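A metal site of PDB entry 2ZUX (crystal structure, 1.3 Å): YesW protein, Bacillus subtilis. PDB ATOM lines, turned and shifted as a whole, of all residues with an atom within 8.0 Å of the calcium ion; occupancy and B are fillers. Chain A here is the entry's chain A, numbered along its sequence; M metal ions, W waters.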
ATOM      1  N   GLN A   4      17.993  16.742  14.182  1.00  0.00           N
ATOM      2  CA  GLN A   4      18.288  16.782  12.761  1.00  0.00           C
ATOM      3  C   GLN A   4      19.270  17.912  12.475  1.00  0.00           C
ATOM      4  O   GLN A   4      19.023  19.066  12.842  1.00  0.00           O
ATOM      5  CB  GLN A   4      17.004  17.000  11.966  1.00  0.00           C
ATOM      6  CG  GLN A   4      17.210  17.084  10.473  1.00  0.00           C
ATOM      7  CD  GLN A   4      16.066  17.801   9.772  1.00  0.00           C
ATOM      8  OE1 GLN A   4      14.913  17.394   9.855  1.00  0.00           O
ATOM      9  NE2 GLN A   4      16.392  18.906   9.106  1.00  0.00           N
ATOM     10  N   ASP A 121      21.907  24.000   1.914  1.00  0.00           N
ATOM     11  CA  ASP A 121      22.362  23.039   0.925  1.00  0.00           C
ATOM     12  C   ASP A 121      21.119  22.585   0.178  1.00  0.00           C
ATOM     13  O   ASP A 121      20.358  21.744   0.664  1.00  0.00           O
ATOM     14  CB  ASP A 121      23.055  21.869   1.613  1.00  0.00           C
ATOM     15  CG  ASP A 121      23.551  20.834   0.647  1.00  0.00           C
ATOM     16  OD1 ASP A 121      23.649  21.111  -0.571  1.00  0.00           O
ATOM     17  OD2 ASP A 121      23.859  19.716   1.114  1.00  0.00           O
ATOM     18  N   VAL A 122      20.879  23.181  -0.989  1.00  0.00           N
ATOM     19  CA  VAL A 122      19.633  22.966  -1.707  1.00  0.00           C
ATOM     20  C   VAL A 122      19.597  21.662  -2.512  1.00  0.00           C
ATOM     21  O   VAL A 122      18.516  21.190  -2.881  1.00  0.00           O
ATOM     22  CB  VAL A 122      19.242  24.147  -2.620  1.00  0.00           C
ATOM     23  CG1 VAL A 122      19.214  25.451  -1.811  1.00  0.00           C
ATOM     24  CG2 VAL A 122      20.182  24.250  -3.819  1.00  0.00           C
ATOM     25  N   TYR A 184      16.264  26.546   5.185  1.00  0.00           N
ATOM     26  CA  TYR A 184      16.455  25.409   6.076  1.00  0.00           C
ATOM     27  C   TYR A 184      15.818  24.179   5.483  1.00  0.00           C
ATOM     28  O   TYR A 184      14.862  24.276   4.719  1.00  0.00           O
ATOM     29  CB  TYR A 184      15.806  25.684   7.455  1.00  0.00           C
ATOM     30  CG  TYR A 184      16.594  25.070   8.587  1.00  0.00           C
ATOM     31  CD1 TYR A 184      17.702  25.720   9.120  1.00  0.00           C
ATOM     32  CD2 TYR A 184      16.248  23.817   9.115  1.00  0.00           C
ATOM     33  CE1 TYR A 184      18.448  25.160  10.135  1.00  0.00           C
ATOM     34  CE2 TYR A 184      16.996  23.247  10.139  1.00  0.00           C
ATOM     35  CZ  TYR A 184      18.088  23.927  10.645  1.00  0.00           C
ATOM     36  OH  TYR A 184      18.869  23.390  11.657  1.00  0.00           O
ATOM     37  N   ASP A 185      16.366  23.018   5.833  1.00  0.00           N
ATOM     38  CA  ASP A 185      15.725  21.752   5.498  1.00  0.00           C
ATOM     39  C   ASP A 185      14.613  21.500   6.515  1.00  0.00           C
ATOM     40  O   ASP A 185      14.818  20.820   7.512  1.00  0.00           O
ATOM     41  CB  ASP A 185      16.750  20.613   5.489  1.00  0.00           C
ATOM     42  CG  ASP A 185      16.141  19.287   5.127  1.00  0.00           C
ATOM     43  OD1 ASP A 185      15.013  19.256   4.591  1.00  0.00           O
ATOM     44  OD2 ASP A 185      16.819  18.265   5.380  1.00  0.00           O
ATOM     45  N   LEU A 186      13.434  22.064   6.244  1.00  0.00           N
ATOM     46  CA  LEU A 186      12.298  21.978   7.153  1.00  0.00           C
ATOM     47  C   LEU A 186      11.708  20.586   7.250  1.00  0.00           C
ATOM     48  O   LEU A 186      11.233  20.196   8.313  1.00  0.00           O
ATOM     49  CB  LEU A 186      11.201  22.958   6.743  1.00  0.00           C
ATOM     50  CG  LEU A 186      11.462  24.442   7.058  1.00  0.00           C
ATOM     51  CD1 LEU A 186      10.491  25.321   6.277  1.00  0.00           C
ATOM     52  CD2 LEU A 186      11.379  24.718   8.540  1.00  0.00           C
ATOM     53  N   ASP A 187      11.702  19.841   6.142  1.00  0.00           N
ATOM     54  CA  ASP A 187      11.030  18.535   6.113  1.00  0.00           C
ATOM     55  C   ASP A 187      11.956  17.331   6.349  1.00  0.00           C
ATOM     56  O   ASP A 187      11.482  16.210   6.531  1.00  0.00           O
ATOM     57  CB  ASP A 187      10.164  18.356   4.855  1.00  0.00           C
ATOM     58  CG  ASP A 187      10.964  18.373   3.568  1.00  0.00           C
ATOM     59  OD1 ASP A 187      12.195  18.502   3.611  1.00  0.00           O
ATOM     60  OD2 ASP A 187      10.329  18.255   2.494  1.00  0.00           O
ATOM     61  N   GLY A 188      13.272  17.578   6.357  1.00  0.00           N
ATOM     62  CA  GLY A 188      14.242  16.552   6.717  1.00  0.00           C
ATOM     63  C   GLY A 188      14.597  15.550   5.631  1.00  0.00           C
ATOM     64  O   GLY A 188      14.953  14.417   5.938  1.00  0.00           O
ATOM     65  N   ASP A 189      14.537  15.983   4.374  1.00  0.00           N
ATOM     66  CA  ASP A 189      14.929  15.112   3.262  1.00  0.00           C
ATOM     67  C   ASP A 189      16.382  15.325   2.819  1.00  0.00           C
ATOM     68  O   ASP A 189      16.857  14.647   1.899  1.00  0.00           O
ATOM     69  CB  ASP A 189      13.987  15.293   2.065  1.00  0.00           C
ATOM     70  CG  ASP A 189      14.209  16.596   1.330  1.00  0.00           C
ATOM     71  OD1 ASP A 189      14.682  17.590   1.952  1.00  0.00           O
ATOM     72  OD2 ASP A 189      13.904  16.636   0.119  1.00  0.00           O
ATOM     73  N   GLY A 190      17.082  16.249   3.481  1.00  0.00           N
ATOM     74  CA  GLY A 190      18.490  16.543   3.190  1.00  0.00           C
ATOM     75  C   GLY A 190      18.723  17.744   2.297  1.00  0.00           C
ATOM     76  O   GLY A 190      19.881  18.094   2.012  1.00  0.00           O
ATOM     77  N   LYS A 191      17.641  18.383   1.853  1.00  0.00           N
ATOM     78  CA  LYS A 191      17.736  19.548   0.973  1.00  0.00           C
ATOM     79  C   LYS A 191      16.999  20.744   1.577  1.00  0.00           C
ATOM     80  O   LYS A 191      15.878  20.604   2.051  1.00  0.00           O
ATOM     81  CB  LYS A 191      17.141  19.230  -0.405  1.00  0.00           C
ATOM     82  CG  LYS A 191      17.927  18.155  -1.168  1.00  0.00           C
ATOM     83  CD  LYS A 191      17.247  17.766  -2.463  1.00  0.00           C
ATOM     84  CE  LYS A 191      17.985  16.633  -3.138  1.00  0.00           C
ATOM     85  NZ  LYS A 191      17.248  16.150  -4.342  1.00  0.00           N
ATOM     86  N   ALA A 192      17.630  21.908   1.538  1.00  0.00           N
ATOM     87  CA  ALA A 192      17.034  23.128   2.068  1.00  0.00           C
ATOM     88  C   ALA A 192      15.910  23.652   1.195  1.00  0.00           C
ATOM     89  O   ALA A 192      15.948  23.540  -0.030  1.00  0.00           O
ATOM     90  CB  ALA A 192      18.086  24.201   2.226  1.00  0.00           C
ATOM     91  N   GLU A 193      14.889  24.197   1.861  1.00  0.00           N
ATOM     92  CA  GLU A 193      13.898  25.024   1.181  1.00  0.00           C
ATOM     93  C   GLU A 193      14.009  26.467   1.680  1.00  0.00           C
ATOM     94  O   GLU A 193      14.800  26.774   2.585  1.00  0.00           O
ATOM     95  CB  GLU A 193      12.473  24.480   1.318  1.00  0.00           C
ATOM     96  CG  GLU A 193      12.171  23.657   2.551  1.00  0.00           C
ATOM     97  CD  GLU A 193      12.691  22.222   2.499  1.00  0.00           C
ATOM     98  OE1 GLU A 193      12.772  21.627   3.590  1.00  0.00           O
ATOM     99  OE2 GLU A 193      13.029  21.692   1.406  1.00  0.00           O
ATOM    100  N   VAL A 194      13.237  27.349   1.050  1.00  0.00           N
ATOM    101  CA  VAL A 194      13.264  28.767   1.373  1.00  0.00           C
ATOM    102  C   VAL A 194      11.838  29.218   1.671  1.00  0.00           C
ATOM    103  O   VAL A 194      10.946  28.994   0.851  1.00  0.00           O
ATOM    104  CB  VAL A 194      13.868  29.604   0.211  1.00  0.00           C
ATOM    105  CG1 VAL A 194      13.942  31.083   0.590  1.00  0.00           C
ATOM    106  CG2 VAL A 194      15.255  29.092  -0.202  1.00  0.00           C
ATOM    107  N   VAL A 233       6.470  28.304   1.010  1.00  0.00           N
ATOM    108  CA  VAL A 233       7.683  27.495   1.052  1.00  0.00           C
ATOM    109  C   VAL A 233       8.070  27.207  -0.394  1.00  0.00           C
ATOM    110  O   VAL A 233       7.258  26.663  -1.156  1.00  0.00           O
ATOM    111  CB  VAL A 233       7.482  26.172   1.826  1.00  0.00           C
ATOM    112  CG1 VAL A 233       8.769  25.366   1.864  1.00  0.00           C
ATOM    113  CG2 VAL A 233       6.977  26.447   3.238  1.00  0.00           C
ATOM    114  N   PHE A 234       9.287  27.578  -0.771  1.00  0.00           N
ATOM    115  CA  PHE A 234       9.823  27.379  -2.117  1.00  0.00           C
ATOM    116  C   PHE A 234      10.856  26.270  -2.090  1.00  0.00           C
ATOM    117  O   PHE A 234      11.642  26.155  -1.131  1.00  0.00           O
ATOM    118  CB  PHE A 234      10.520  28.647  -2.621  1.00  0.00           C
ATOM    119  CG  PHE A 234       9.625  29.851  -2.783  1.00  0.00           C
ATOM    120  CD1 PHE A 234       8.922  30.076  -3.970  1.00  0.00           C
ATOM    121  CD2 PHE A 234       9.529  30.797  -1.764  1.00  0.00           C
ATOM    122  CE1 PHE A 234       8.134  31.209  -4.134  1.00  0.00           C
ATOM    123  CE2 PHE A 234       8.741  31.930  -1.927  1.00  0.00           C
ATOM    124  CZ  PHE A 234       8.034  32.132  -3.109  1.00  0.00           C
ATOM    125  N   GLN A 235      10.899  25.481  -3.150  1.00  0.00           N
ATOM    126  CA  GLN A 235      11.905  24.441  -3.317  1.00  0.00           C
ATOM    127  C   GLN A 235      13.278  25.084  -3.443  1.00  0.00           C
ATOM    128  O   GLN A 235      13.463  26.010  -4.222  1.00  0.00           O
ATOM    129  CB  GLN A 235      11.577  23.610  -4.570  1.00  0.00           C
ATOM    130  CG  GLN A 235      12.479  22.416  -4.783  1.00  0.00           C
ATOM    131  CD  GLN A 235      12.003  21.531  -5.916  1.00  0.00           C
ATOM    132  OE1 GLN A 235      11.680  22.014  -6.996  1.00  0.00           O
ATOM    133  NE2 GLN A 235      11.964  20.236  -5.671  1.00  0.00           N
ATOM    134  N   GLY A 236      14.239  24.614  -2.658  1.00  0.00           N
ATOM    135  CA  GLY A 236      15.557  25.231  -2.640  1.00  0.00           C
ATOM    136  C   GLY A 236      16.328  25.176  -3.942  1.00  0.00           C
ATOM    137  O   GLY A 236      17.052  26.102  -4.275  1.00  0.00           O
ATOM    138  N   LEU A 242       6.221  25.450  -3.513  1.00  0.00           N
ATOM    139  CA  LEU A 242       5.777  24.132  -3.045  1.00  0.00           C
ATOM    140  C   LEU A 242       4.389  24.201  -2.408  1.00  0.00           C
ATOM    141  O   LEU A 242       3.505  23.417  -2.739  1.00  0.00           O
ATOM    142  CB  LEU A 242       6.780  23.514  -2.077  1.00  0.00           C
ATOM    143  CG  LEU A 242       8.134  23.120  -2.667  1.00  0.00           C
ATOM    144  CD1 LEU A 242       9.100  22.694  -1.559  1.00  0.00           C
ATOM    145  CD2 LEU A 242       7.971  21.997  -3.708  1.00  0.00           C
ATOM    146  N   PHE A 299       6.744  22.351   8.158  1.00  0.00           N
ATOM    147  CA  PHE A 299       6.630  21.914   6.775  1.00  0.00           C
ATOM    148  C   PHE A 299       7.226  20.517   6.705  1.00  0.00           C
ATOM    149  O   PHE A 299       8.432  20.339   6.767  1.00  0.00           O
ATOM    150  CB  PHE A 299       7.332  22.865   5.793  1.00  0.00           C
ATOM    151  CG  PHE A 299       7.303  22.375   4.378  1.00  0.00           C
ATOM    152  CD1 PHE A 299       6.109  22.370   3.648  1.00  0.00           C
ATOM    153  CD2 PHE A 299       8.456  21.886   3.774  1.00  0.00           C
ATOM    154  CE1 PHE A 299       6.070  21.893   2.346  1.00  0.00           C
ATOM    155  CE2 PHE A 299       8.430  21.404   2.463  1.00  0.00           C
ATOM    156  CZ  PHE A 299       7.229  21.417   1.745  1.00  0.00           C
ATOM    157  N   PRO A 583      19.710  13.627   7.814  1.00  0.00           N
ATOM    158  CA  PRO A 583      18.813  12.902   6.922  1.00  0.00           C
ATOM    159  C   PRO A 583      19.547  11.851   6.097  1.00  0.00           C
ATOM    160  O   PRO A 583      18.961  10.814   5.764  1.00  0.00           O
ATOM    161  CB  PRO A 583      18.274  14.013   6.015  1.00  0.00           C
ATOM    162  CG  PRO A 583      18.350  15.241   6.852  1.00  0.00           C
ATOM    163  CD  PRO A 583      19.616  15.095   7.616  1.00  0.00           C
HETATM  164 CA    CA M   1      13.852  19.645   2.483  1.00  0.00          CA
HETATM  165  O   HOH W   1      13.169  19.144   0.183  1.00  0.00           O
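The side-chain carboxylate (OE1) of Glu 193 sits close to the backbone NH (N) of Leu 186 (2.8 Å). O of Tyr 184 is in hydrogen-bond range of N of Glu 193, 2.9 Å away. The backbone NH (N) of Asp 187 sits close to the backbone carbonyl oxygen (O) of Phe 299, 3.4 Å away. N of Gly 190 sits at hydrogen-bond distance from OD2 of Asp 185, 2.8 Å away. The side-chain carboxylate of Asp 185 lies close to the backbone NH of Gly 188 (3.0 Å). O of Asp 185 is in hydrogen-bond range of NE2 of Gln 4 (2.9 Å).
Of the 21 residues printed, 5 come within 4 Å of the calcium ion.
The calcium ion is bound by OD1 of Asp 189 (2.3 Å), O of Lys 191 (2.3 Å), OD1 of Asp 187 (2.3 Å), OD1 of Asp 185 (2.4 Å), water W1 (2.5 Å), OE2 of Glu 193 (2.5 Å) and OE1 of Glu 193 (2.5 Å). The calcium ion has seven donor atoms within binding distance.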
